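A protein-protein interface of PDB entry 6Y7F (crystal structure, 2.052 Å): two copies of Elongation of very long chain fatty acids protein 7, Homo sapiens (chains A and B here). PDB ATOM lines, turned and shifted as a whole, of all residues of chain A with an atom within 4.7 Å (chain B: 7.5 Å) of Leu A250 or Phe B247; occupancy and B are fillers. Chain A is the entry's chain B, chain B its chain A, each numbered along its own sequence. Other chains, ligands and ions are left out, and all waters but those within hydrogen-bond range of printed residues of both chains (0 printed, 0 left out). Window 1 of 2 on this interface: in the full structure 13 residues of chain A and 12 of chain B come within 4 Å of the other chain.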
ATOM      1  N   LEU A 212      -4.922 -11.270 -40.357  1.00  0.00           N
ATOM      2  CA  LEU A 212      -4.665 -10.908 -38.965  1.00  0.00           C
ATOM      3  C   LEU A 212      -5.953 -10.448 -38.253  1.00  0.00           C
ATOM      4  O   LEU A 212      -6.202 -10.851 -37.120  1.00  0.00           O
ATOM      5  CB  LEU A 212      -3.616  -9.800 -38.892  1.00  0.00           C
ATOM      6  CG  LEU A 212      -2.203 -10.243 -39.187  1.00  0.00           C
ATOM      7  CD1 LEU A 212      -1.318  -9.059 -39.456  1.00  0.00           C
ATOM      8  CD2 LEU A 212      -1.659 -11.055 -38.061  1.00  0.00           C
ATOM      9  N   PHE A 215      -8.175 -13.366 -37.199  1.00  0.00           N
ATOM     10  CA  PHE A 215      -7.818 -14.029 -35.938  1.00  0.00           C
ATOM     11  C   PHE A 215      -8.260 -13.186 -34.741  1.00  0.00           C
ATOM     12  O   PHE A 215      -8.804 -13.736 -33.782  1.00  0.00           O
ATOM     13  CB  PHE A 215      -6.307 -14.324 -35.846  1.00  0.00           C
ATOM     14  CG  PHE A 215      -5.805 -15.087 -37.050  1.00  0.00           C
ATOM     15  CD1 PHE A 215      -6.489 -16.185 -37.531  1.00  0.00           C
ATOM     16  CD2 PHE A 215      -4.645 -14.703 -37.697  1.00  0.00           C
ATOM     17  CE1 PHE A 215      -6.044 -16.860 -38.663  1.00  0.00           C
ATOM     18  CE2 PHE A 215      -4.212 -15.371 -38.828  1.00  0.00           C
ATOM     19  CZ  PHE A 215      -4.914 -16.442 -39.310  1.00  0.00           C
ATOM     20  N   VAL A 216      -8.123 -11.864 -34.837  1.00  0.00           N
ATOM     21  CA  VAL A 216      -8.570 -10.970 -33.765  1.00  0.00           C
ATOM     22  C   VAL A 216     -10.103 -11.106 -33.550  1.00  0.00           C
ATOM     23  O   VAL A 216     -10.530 -11.302 -32.414  1.00  0.00           O
ATOM     24  CB  VAL A 216      -8.173  -9.495 -34.008  1.00  0.00           C
ATOM     25  CG1 VAL A 216      -8.814  -8.576 -32.958  1.00  0.00           C
ATOM     26  CG2 VAL A 216      -6.643  -9.326 -34.019  1.00  0.00           C
ATOM     27  N   SER A 246      -6.370 -19.355 -32.420  1.00  0.00           N
ATOM     28  CA  SER A 246      -6.403 -18.006 -32.982  1.00  0.00           C
ATOM     29  C   SER A 246      -5.236 -17.159 -32.450  1.00  0.00           C
ATOM     30  O   SER A 246      -4.706 -16.358 -33.201  1.00  0.00           O
ATOM     31  CB  SER A 246      -7.746 -17.328 -32.729  1.00  0.00           C
ATOM     32  OG  SER A 246      -7.818 -16.781 -31.420  1.00  0.00           O
ATOM     33  N   PHE A 247      -4.762 -17.410 -31.223  1.00  0.00           N
ATOM     34  CA  PHE A 247      -3.563 -16.739 -30.657  1.00  0.00           C
ATOM     35  C   PHE A 247      -2.287 -17.294 -31.307  1.00  0.00           C
ATOM     36  O   PHE A 247      -1.371 -16.528 -31.611  1.00  0.00           O
ATOM     37  CB  PHE A 247      -3.460 -16.930 -29.130  1.00  0.00           C
ATOM     38  CG  PHE A 247      -4.405 -16.147 -28.260  1.00  0.00           C
ATOM     39  CD1 PHE A 247      -5.108 -15.071 -28.764  1.00  0.00           C
ATOM     40  CD2 PHE A 247      -4.569 -16.472 -26.917  1.00  0.00           C
ATOM     41  CE1 PHE A 247      -5.951 -14.321 -27.932  1.00  0.00           C
ATOM     42  CE2 PHE A 247      -5.429 -15.741 -26.101  1.00  0.00           C
ATOM     43  CZ  PHE A 247      -6.115 -14.671 -26.610  1.00  0.00           C
ATOM     44  N   MET A 248      -2.214 -18.624 -31.503  1.00  0.00           N
ATOM     45  CA  MET A 248      -1.060 -19.235 -32.158  1.00  0.00           C
ATOM     46  C   MET A 248      -0.890 -18.710 -33.586  1.00  0.00           C
ATOM     47  O   MET A 248       0.220 -18.425 -33.993  1.00  0.00           O
ATOM     48  CB  MET A 248      -1.175 -20.769 -32.212  1.00  0.00           C
ATOM     49  CG  MET A 248      -0.776 -21.477 -30.938  1.00  0.00           C
ATOM     50  SD  MET A 248      -1.348 -23.202 -31.087  1.00  0.00           S
ATOM     51  CE  MET A 248      -0.242 -23.976 -29.902  1.00  0.00           C
ATOM     52  N   PHE A 249      -1.988 -18.598 -34.345  1.00  0.00           N
ATOM     53  CA  PHE A 249      -1.914 -18.118 -35.721  1.00  0.00           C
ATOM     54  C   PHE A 249      -1.655 -16.629 -35.772  1.00  0.00           C
ATOM     55  O   PHE A 249      -0.980 -16.183 -36.669  1.00  0.00           O
ATOM     56  CB  PHE A 249      -3.170 -18.475 -36.511  1.00  0.00           C
ATOM     57  CG  PHE A 249      -3.266 -19.962 -36.703  1.00  0.00           C
ATOM     58  CD1 PHE A 249      -2.184 -20.688 -37.162  1.00  0.00           C
ATOM     59  CD2 PHE A 249      -4.435 -20.640 -36.417  1.00  0.00           C
ATOM     60  CE1 PHE A 249      -2.269 -22.070 -37.316  1.00  0.00           C
ATOM     61  CE2 PHE A 249      -4.513 -22.017 -36.568  1.00  0.00           C
ATOM     62  CZ  PHE A 249      -3.435 -22.721 -37.031  1.00  0.00           C
ATOM     63  N   LEU A 250      -2.179 -15.860 -34.830  1.00  0.00           N
ATOM     64  CA  LEU A 250      -1.929 -14.421 -34.772  1.00  0.00           C
ATOM     65  C   LEU A 250      -0.424 -14.157 -34.587  1.00  0.00           C
ATOM     66  O   LEU A 250       0.138 -13.354 -35.310  1.00  0.00           O
ATOM     67  CB  LEU A 250      -2.749 -13.822 -33.636  1.00  0.00           C
ATOM     68  CG  LEU A 250      -2.922 -12.313 -33.548  1.00  0.00           C
ATOM     69  CD1 LEU A 250      -3.164 -11.663 -34.917  1.00  0.00           C
ATOM     70  CD2 LEU A 250      -4.125 -11.987 -32.603  1.00  0.00           C
ATOM     71  N   LEU A 251       0.245 -14.967 -33.765  1.00  0.00           N
ATOM     72  CA  LEU A 251       1.674 -14.878 -33.507  1.00  0.00           C
ATOM     73  C   LEU A 251       2.490 -15.321 -34.717  1.00  0.00           C
ATOM     74  O   LEU A 251       3.481 -14.656 -35.084  1.00  0.00           O
ATOM     75  CB  LEU A 251       2.005 -15.742 -32.297  1.00  0.00           C
ATOM     76  CG  LEU A 251       3.455 -15.830 -31.907  1.00  0.00           C
ATOM     77  CD1 LEU A 251       3.877 -14.607 -31.077  1.00  0.00           C
ATOM     78  CD2 LEU A 251       3.713 -17.110 -31.122  1.00  0.00           C
ATOM     79  N   LEU A 252       2.081 -16.439 -35.359  1.00  0.00           N
ATOM     80  CA  LEU A 252       2.757 -16.930 -36.543  1.00  0.00           C
ATOM     81  C   LEU A 252       2.603 -15.924 -37.689  1.00  0.00           C
ATOM     82  O   LEU A 252       3.580 -15.644 -38.373  1.00  0.00           O
ATOM     83  CB  LEU A 252       2.195 -18.307 -36.954  1.00  0.00           C
ATOM     84  CG  LEU A 252       2.599 -19.459 -36.041  1.00  0.00           C
ATOM     85  CD1 LEU A 252       1.743 -20.680 -36.268  1.00  0.00           C
ATOM     86  CD2 LEU A 252       4.094 -19.759 -36.142  1.00  0.00           C
ATOM     87  N   PHE A 253       1.395 -15.350 -37.885  1.00  0.00           N
ATOM     88  CA  PHE A 253       1.193 -14.373 -38.968  1.00  0.00           C
ATOM     89  C   PHE A 253       1.885 -13.025 -38.670  1.00  0.00           C
ATOM     90  O   PHE A 253       2.283 -12.345 -39.613  1.00  0.00           O
ATOM     91  CB  PHE A 253      -0.285 -14.151 -39.281  1.00  0.00           C
ATOM     92  CG  PHE A 253      -0.843 -15.162 -40.256  1.00  0.00           C
ATOM     93  CD1 PHE A 253      -1.100 -16.464 -39.858  1.00  0.00           C
ATOM     94  CD2 PHE A 253      -1.066 -14.823 -41.583  1.00  0.00           C
ATOM     95  CE1 PHE A 253      -1.625 -17.403 -40.771  1.00  0.00           C
ATOM     96  CE2 PHE A 253      -1.590 -15.761 -42.489  1.00  0.00           C
ATOM     97  CZ  PHE A 253      -1.845 -17.045 -42.081  1.00  0.00           C
ATOM     98  N   LEU A 254       2.043 -12.654 -37.398  1.00  0.00           N
ATOM     99  CA  LEU A 254       2.786 -11.432 -37.067  1.00  0.00           C
ATOM    100  C   LEU A 254       4.271 -11.679 -37.365  1.00  0.00           C
ATOM    101  O   LEU A 254       4.923 -10.795 -37.915  1.00  0.00           O
ATOM    102  CB  LEU A 254       2.562 -10.952 -35.618  1.00  0.00           C
ATOM    103  CG  LEU A 254       1.175 -10.316 -35.388  1.00  0.00           C
ATOM    104  CD1 LEU A 254       0.835 -10.252 -33.964  1.00  0.00           C
ATOM    105  CD2 LEU A 254       1.090  -8.932 -35.963  1.00  0.00           C
ATOM    106  N   PHE B 215      -2.995  -7.757 -19.964  1.00  0.00           N
ATOM    107  CA  PHE B 215      -2.420  -8.654 -20.981  1.00  0.00           C
ATOM    108  C   PHE B 215      -2.768  -8.155 -22.394  1.00  0.00           C
ATOM    109  O   PHE B 215      -1.904  -8.162 -23.280  1.00  0.00           O
ATOM    110  CB  PHE B 215      -2.900 -10.106 -20.802  1.00  0.00           C
ATOM    111  CG  PHE B 215      -2.674 -10.621 -19.402  1.00  0.00           C
ATOM    112  CD1 PHE B 215      -1.462 -10.422 -18.760  1.00  0.00           C
ATOM    113  CD2 PHE B 215      -3.677 -11.301 -18.722  1.00  0.00           C
ATOM    114  CE1 PHE B 215      -1.266 -10.857 -17.445  1.00  0.00           C
ATOM    115  CE2 PHE B 215      -3.477 -11.729 -17.409  1.00  0.00           C
ATOM    116  CZ  PHE B 215      -2.274 -11.495 -16.775  1.00  0.00           C
ATOM    117  N   VAL B 216      -3.993  -7.646 -22.589  1.00  0.00           N
ATOM    118  CA  VAL B 216      -4.381  -7.083 -23.883  1.00  0.00           C
ATOM    119  C   VAL B 216      -3.486  -5.880 -24.247  1.00  0.00           C
ATOM    120  O   VAL B 216      -2.946  -5.851 -25.344  1.00  0.00           O
ATOM    121  CB  VAL B 216      -5.883  -6.694 -23.941  1.00  0.00           C
ATOM    122  CG1 VAL B 216      -6.199  -5.964 -25.247  1.00  0.00           C
ATOM    123  CG2 VAL B 216      -6.780  -7.933 -23.791  1.00  0.00           C
ATOM    124  N   VAL B 218      -0.468  -5.141 -23.132  1.00  0.00           N
ATOM    125  CA  VAL B 218       0.888  -5.646 -23.321  1.00  0.00           C
ATOM    126  C   VAL B 218       1.037  -6.237 -24.730  1.00  0.00           C
ATOM    127  O   VAL B 218       2.046  -5.976 -25.400  1.00  0.00           O
ATOM    128  CB  VAL B 218       1.263  -6.665 -22.221  1.00  0.00           C
ATOM    129  CG1 VAL B 218       2.525  -7.453 -22.589  1.00  0.00           C
ATOM    130  CG2 VAL B 218       1.443  -5.952 -20.879  1.00  0.00           C
ATOM    131  N   ALA B 219       0.029  -7.006 -25.186  1.00  0.00           N
ATOM    132  CA  ALA B 219       0.042  -7.601 -26.515  1.00  0.00           C
ATOM    133  C   ALA B 219      -0.052  -6.517 -27.574  1.00  0.00           C
ATOM    134  O   ALA B 219       0.618  -6.627 -28.583  1.00  0.00           O
ATOM    135  CB  ALA B 219      -1.121  -8.593 -26.676  1.00  0.00           C
ATOM    136  N   ILE B 220      -0.922  -5.502 -27.394  1.00  0.00           N
ATOM    137  CA  ILE B 220      -1.072  -4.436 -28.390  1.00  0.00           C
ATOM    138  C   ILE B 220       0.240  -3.634 -28.486  1.00  0.00           C
ATOM    139  O   ILE B 220       0.683  -3.329 -29.594  1.00  0.00           O
ATOM    140  CB  ILE B 220      -2.283  -3.527 -28.056  1.00  0.00           C
ATOM    141  CG1 ILE B 220      -3.612  -4.301 -28.216  1.00  0.00           C
ATOM    142  CG2 ILE B 220      -2.278  -2.251 -28.923  1.00  0.00           C
ATOM    143  CD1 ILE B 220      -4.812  -3.534 -27.717  1.00  0.00           C
ATOM    144  N   ILE B 222       3.483  -4.669 -27.644  1.00  0.00           N
ATOM    145  CA  ILE B 222       4.556  -5.465 -28.225  1.00  0.00           C
ATOM    146  C   ILE B 222       4.283  -5.802 -29.690  1.00  0.00           C
ATOM    147  O   ILE B 222       5.244  -6.003 -30.424  1.00  0.00           O
ATOM    148  CB  ILE B 222       4.827  -6.741 -27.403  1.00  0.00           C
ATOM    149  CG1 ILE B 222       6.275  -7.198 -27.566  1.00  0.00           C
ATOM    150  CG2 ILE B 222       3.834  -7.867 -27.733  1.00  0.00           C
ATOM    151  CD1 ILE B 222       7.298  -6.235 -26.881  1.00  0.00           C
ATOM    152  N   SER B 223       2.993  -5.837 -30.132  1.00  0.00           N
ATOM    153  CA  SER B 223       2.679  -6.136 -31.542  1.00  0.00           C
ATOM    154  C   SER B 223       3.259  -5.061 -32.492  1.00  0.00           C
ATOM    155  O   SER B 223       3.512  -5.375 -33.649  1.00  0.00           O
ATOM    156  CB  SER B 223       1.177  -6.282 -31.768  1.00  0.00           C
ATOM    157  OG  SER B 223       0.521  -5.025 -31.779  1.00  0.00           O
ATOM    158  N   PHE B 226       6.533  -5.960 -34.664  1.00  0.00           N
ATOM    159  CA  PHE B 226       6.434  -6.691 -35.928  1.00  0.00           C
ATOM    160  C   PHE B 226       6.218  -5.768 -37.130  1.00  0.00           C
ATOM    161  O   PHE B 226       6.526  -6.171 -38.251  1.00  0.00           O
ATOM    162  CB  PHE B 226       5.290  -7.742 -35.854  1.00  0.00           C
ATOM    163  CG  PHE B 226       5.485  -8.683 -34.684  1.00  0.00           C
ATOM    164  CD1 PHE B 226       6.362  -9.750 -34.773  1.00  0.00           C
ATOM    165  CD2 PHE B 226       4.875  -8.436 -33.463  1.00  0.00           C
ATOM    166  CE1 PHE B 226       6.593 -10.569 -33.676  1.00  0.00           C
ATOM    167  CE2 PHE B 226       5.125  -9.247 -32.366  1.00  0.00           C
ATOM    168  CZ  PHE B 226       5.987 -10.301 -32.474  1.00  0.00           C
ATOM    169  N   CYS B 240       8.644 -11.780 -29.337  1.00  0.00           N
ATOM    170  CA  CYS B 240       7.887 -13.021 -29.480  1.00  0.00           C
ATOM    171  C   CYS B 240       7.564 -13.640 -28.144  1.00  0.00           C
ATOM    172  O   CYS B 240       6.481 -14.212 -27.994  1.00  0.00           O
ATOM    173  CB  CYS B 240       8.630 -14.008 -30.367  1.00  0.00           C
ATOM    174  SG  CYS B 240       8.661 -13.521 -32.098  1.00  0.00           S
ATOM    175  N   ILE B 241       8.496 -13.576 -27.196  1.00  0.00           N
ATOM    176  CA  ILE B 241       8.271 -14.141 -25.880  1.00  0.00           C
ATOM    177  C   ILE B 241       7.185 -13.338 -25.164  1.00  0.00           C
ATOM    178  O   ILE B 241       6.214 -13.914 -24.698  1.00  0.00           O
ATOM    179  CB  ILE B 241       9.607 -14.197 -25.086  1.00  0.00           C
ATOM    180  CG1 ILE B 241      10.519 -15.314 -25.680  1.00  0.00           C
ATOM    181  CG2 ILE B 241       9.379 -14.385 -23.578  1.00  0.00           C
ATOM    182  CD1 ILE B 241      11.988 -15.086 -25.323  1.00  0.00           C
ATOM    183  N   ILE B 242       7.321 -12.013 -25.112  1.00  0.00           N
ATOM    184  CA  ILE B 242       6.330 -11.144 -24.477  1.00  0.00           C
ATOM    185  C   ILE B 242       4.909 -11.356 -25.087  1.00  0.00           C
ATOM    186  O   ILE B 242       3.953 -11.526 -24.339  1.00  0.00           O
ATOM    187  CB  ILE B 242       6.793  -9.684 -24.588  1.00  0.00           C
ATOM    188  CG1 ILE B 242       8.095  -9.461 -23.769  1.00  0.00           C
ATOM    189  CG2 ILE B 242       5.705  -8.732 -24.124  1.00  0.00           C
ATOM    190  CD1 ILE B 242       8.786  -8.175 -24.069  1.00  0.00           C
ATOM    191  N   MET B 243       4.795 -11.382 -26.417  1.00  0.00           N
ATOM    192  CA  MET B 243       3.543 -11.572 -27.148  1.00  0.00           C
ATOM    193  C   MET B 243       2.917 -12.925 -26.800  1.00  0.00           C
ATOM    194  O   MET B 243       1.743 -12.962 -26.442  1.00  0.00           O
ATOM    195  CB  MET B 243       3.811 -11.454 -28.657  1.00  0.00           C
ATOM    196  CG  MET B 243       2.573 -11.597 -29.521  1.00  0.00           C
ATOM    197  SD  MET B 243       1.507 -10.137 -29.487  1.00  0.00           S
ATOM    198  CE  MET B 243       1.483  -9.787 -31.063  1.00  0.00           C
ATOM    199  N   SER B 244       3.708 -14.026 -26.858  1.00  0.00           N
ATOM    200  CA  SER B 244       3.211 -15.359 -26.550  1.00  0.00           C
ATOM    201  C   SER B 244       2.830 -15.509 -25.080  1.00  0.00           C
ATOM    202  O   SER B 244       1.821 -16.151 -24.799  1.00  0.00           O
ATOM    203  CB  SER B 244       4.236 -16.421 -26.925  1.00  0.00           C
ATOM    204  OG  SER B 244       5.406 -16.273 -26.141  1.00  0.00           O
ATOM    205  N   TYR B 245       3.632 -14.950 -24.140  1.00  0.00           N
ATOM    206  CA  TYR B 245       3.315 -15.070 -22.712  1.00  0.00           C
ATOM    207  C   TYR B 245       2.034 -14.323 -22.387  1.00  0.00           C
ATOM    208  O   TYR B 245       1.205 -14.851 -21.656  1.00  0.00           O
ATOM    209  CB  TYR B 245       4.444 -14.563 -21.812  1.00  0.00           C
ATOM    210  CG  TYR B 245       5.618 -15.503 -21.619  1.00  0.00           C
ATOM    211  CD1 TYR B 245       5.910 -16.498 -22.554  1.00  0.00           C
ATOM    212  CD2 TYR B 245       6.482 -15.352 -20.539  1.00  0.00           C
ATOM    213  CE1 TYR B 245       7.036 -17.316 -22.417  1.00  0.00           C
ATOM    214  CE2 TYR B 245       7.575 -16.193 -20.366  1.00  0.00           C
ATOM    215  CZ  TYR B 245       7.874 -17.146 -21.324  1.00  0.00           C
ATOM    216  OH  TYR B 245       8.964 -17.957 -21.114  1.00  0.00           O
ATOM    217  N   SER B 246       1.825 -13.131 -22.961  1.00  0.00           N
ATOM    218  CA  SER B 246       0.609 -12.365 -22.696  1.00  0.00           C
ATOM    219  C   SER B 246      -0.610 -13.127 -23.235  1.00  0.00           C
ATOM    220  O   SER B 246      -1.621 -13.161 -22.552  1.00  0.00           O
ATOM    221  CB  SER B 246       0.709 -10.942 -23.244  1.00  0.00           C
ATOM    222  OG  SER B 246       0.539 -10.903 -24.647  1.00  0.00           O
ATOM    223  N   PHE B 247      -0.477 -13.860 -24.364  1.00  0.00           N
ATOM    224  CA  PHE B 247      -1.549 -14.718 -24.889  1.00  0.00           C
ATOM    225  C   PHE B 247      -1.771 -15.910 -23.962  1.00  0.00           C
ATOM    226  O   PHE B 247      -2.919 -16.276 -23.712  1.00  0.00           O
ATOM    227  CB  PHE B 247      -1.230 -15.241 -26.303  1.00  0.00           C
ATOM    228  CG  PHE B 247      -1.357 -14.279 -27.461  1.00  0.00           C
ATOM    229  CD1 PHE B 247      -1.995 -13.056 -27.305  1.00  0.00           C
ATOM    230  CD2 PHE B 247      -0.786 -14.568 -28.690  1.00  0.00           C
ATOM    231  CE1 PHE B 247      -2.129 -12.182 -28.384  1.00  0.00           C
ATOM    232  CE2 PHE B 247      -0.925 -13.698 -29.762  1.00  0.00           C
ATOM    233  CZ  PHE B 247      -1.605 -12.519 -29.611  1.00  0.00           C
ATOM    234  N   MET B 248      -0.690 -16.550 -23.471  1.00  0.00           N
ATOM    235  CA  MET B 248      -0.819 -17.685 -22.541  1.00  0.00           C
ATOM    236  C   MET B 248      -1.546 -17.279 -21.257  1.00  0.00           C
ATOM    237  O   MET B 248      -2.420 -18.017 -20.799  1.00  0.00           O
ATOM    238  CB  MET B 248       0.545 -18.270 -22.158  1.00  0.00           C
ATOM    239  CG  MET B 248       1.128 -19.227 -23.187  1.00  0.00           C
ATOM    240  SD  MET B 248       2.885 -19.493 -22.767  1.00  0.00           S
ATOM    241  CE  MET B 248       3.106 -21.081 -23.523  1.00  0.00           C
ATOM    242  N   PHE B 249      -1.194 -16.110 -20.683  1.00  0.00           N
ATOM    243  CA  PHE B 249      -1.833 -15.660 -19.460  1.00  0.00           C
ATOM    244  C   PHE B 249      -3.248 -15.184 -19.715  1.00  0.00           C
ATOM    245  O   PHE B 249      -4.097 -15.372 -18.865  1.00  0.00           O
ATOM    246  CB  PHE B 249      -1.016 -14.559 -18.759  1.00  0.00           C
ATOM    247  CG  PHE B 249       0.289 -15.115 -18.262  1.00  0.00           C
ATOM    248  CD1 PHE B 249       0.324 -16.277 -17.517  1.00  0.00           C
ATOM    249  CD2 PHE B 249       1.491 -14.476 -18.541  1.00  0.00           C
ATOM    250  CE1 PHE B 249       1.544 -16.809 -17.085  1.00  0.00           C
ATOM    251  CE2 PHE B 249       2.704 -15.015 -18.111  1.00  0.00           C
ATOM    252  CZ  PHE B 249       2.722 -16.179 -17.388  1.00  0.00           C
ATOM    253  N   LEU B 250      -3.518 -14.580 -20.873  1.00  0.00           N
ATOM    254  CA  LEU B 250      -4.865 -14.137 -21.210  1.00  0.00           C
ATOM    255  C   LEU B 250      -5.812 -15.356 -21.276  1.00  0.00           C
ATOM    256  O   LEU B 250      -6.887 -15.311 -20.702  1.00  0.00           O
ATOM    257  CB  LEU B 250      -4.807 -13.389 -22.540  1.00  0.00           C
ATOM    258  CG  LEU B 250      -6.014 -12.587 -23.022  1.00  0.00           C
ATOM    259  CD1 LEU B 250      -6.627 -11.774 -21.902  1.00  0.00           C
ATOM    260  CD2 LEU B 250      -5.571 -11.631 -24.148  1.00  0.00           C
ATOM    261  N   LEU B 251      -5.332 -16.485 -21.800  1.00  0.00           N
ATOM    262  CA  LEU B 251      -6.096 -17.729 -21.888  1.00  0.00           C
ATOM    263  C   LEU B 251      -6.279 -18.374 -20.501  1.00  0.00           C
ATOM    264  O   LEU B 251      -7.377 -18.829 -20.166  1.00  0.00           O
ATOM    265  CB  LEU B 251      -5.369 -18.671 -22.833  1.00  0.00           C
ATOM    266  CG  LEU B 251      -5.938 -20.049 -22.985  1.00  0.00           C
ATOM    267  CD1 LEU B 251      -7.173 -20.066 -23.937  1.00  0.00           C
ATOM    268  CD2 LEU B 251      -4.864 -21.008 -23.490  1.00  0.00           C
ATOM    269  N   LEU B 252      -5.208 -18.403 -19.699  1.00  0.00           N
ATOM    270  CA  LEU B 252      -5.274 -18.936 -18.343  1.00  0.00           C
ATOM    271  C   LEU B 252      -6.206 -18.088 -17.472  1.00  0.00           C
ATOM    272  O   LEU B 252      -7.025 -18.657 -16.759  1.00  0.00           O
ATOM    273  CB  LEU B 252      -3.885 -19.010 -17.700  1.00  0.00           C
ATOM    274  CG  LEU B 252      -2.972 -20.099 -18.275  1.00  0.00           C
ATOM    275  CD1 LEU B 252      -1.522 -19.864 -17.863  1.00  0.00           C
ATOM    276  CD2 LEU B 252      -3.461 -21.480 -17.894  1.00  0.00           C
ATOM    277  N   PHE B 253      -6.140 -16.752 -17.571  1.00  0.00           N
ATOM    278  CA  PHE B 253      -7.017 -15.875 -16.782  1.00  0.00           C
ATOM    279  C   PHE B 253      -8.466 -15.911 -17.289  1.00  0.00           C
ATOM    280  O   PHE B 253      -9.377 -15.729 -16.480  1.00  0.00           O
ATOM    281  CB  PHE B 253      -6.513 -14.438 -16.725  1.00  0.00           C
ATOM    282  CG  PHE B 253      -5.500 -14.210 -15.625  1.00  0.00           C
ATOM    283  CD1 PHE B 253      -4.204 -14.693 -15.738  1.00  0.00           C
ATOM    284  CD2 PHE B 253      -5.857 -13.554 -14.454  1.00  0.00           C
ATOM    285  CE1 PHE B 253      -3.270 -14.467 -14.724  1.00  0.00           C
ATOM    286  CE2 PHE B 253      -4.926 -13.342 -13.444  1.00  0.00           C
ATOM    287  CZ  PHE B 253      -3.645 -13.810 -13.579  1.00  0.00           C
ATOM    288  N   LEU B 254      -8.693 -16.152 -18.588  1.00  0.00           N
ATOM    289  CA  LEU B 254     -10.068 -16.312 -19.089  1.00  0.00           C
ATOM    290  C   LEU B 254     -10.622 -17.631 -18.564  1.00  0.00           C
ATOM    291  O   LEU B 254     -11.766 -17.644 -18.134  1.00  0.00           O
ATOM    292  CB  LEU B 254     -10.178 -16.219 -20.616  1.00  0.00           C
ATOM    293  CG  LEU B 254     -10.007 -14.790 -21.173  1.00  0.00           C
ATOM    294  CD1 LEU B 254      -9.683 -14.829 -22.637  1.00  0.00           C
ATOM    295  CD2 LEU B 254     -11.245 -13.935 -20.916  1.00  0.00           C
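The side-chain hydroxyl (OG) of Ser B246 is in hydrogen-bond range of the backbone carbonyl oxygen (O) of Met B243 (3.0 Å).
Among the printed residues, pairs that only touch across the chains: Phe A247 with Phe B247 (3.4 Å), Phe A247 with Leu B250 (3.9 Å), Leu A250 with Phe B247 (3.9 Å), Leu A251 with Met B243 (3.6 Å), Leu A254 with Phe B226 (3.6 Å) and Leu A254 with Met B243 (3.0 Å).
Printed residues of chain B within 4 Å of Leu A251: Met B243 (3.6 Å).
Of the printed residues of chain B, Leu A254 touches Phe B226 (3.6 Å) and Met B243 (3.0 Å).
Ser B223 touches none of the printed residues of chain A.
Of the printed residues of chain A, Met B243 touches Leu A251 and Leu A254.
Ser B244 touches none of the printed residues of chain A.
Phe B247 touches two residues of chain A.
Printed residues of chain A within 4 Å of Leu B250: Phe A247.
The nearest residue of chain B that does not touch Leu A250 is Met B243 (5.7 Å).
Of the 23 printed residues of chain B, 4 touch a printed residue of chain A.
Hydrophobic or aromatic side chains of chain B that line the printed part of chain A: Phe B226, Met B243, Phe B247 and Leu B250.
Hydrophobic or aromatic side chains of chain A within 4 Å of the printed part of chain B: Phe A247, Leu A250, Leu A251 and Leu A254.
Phe A247 touches its own counterpart, Phe B247.
Phe A247 touches Leu B250, and with the chains exchanged Leu A250 touches Phe B247.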
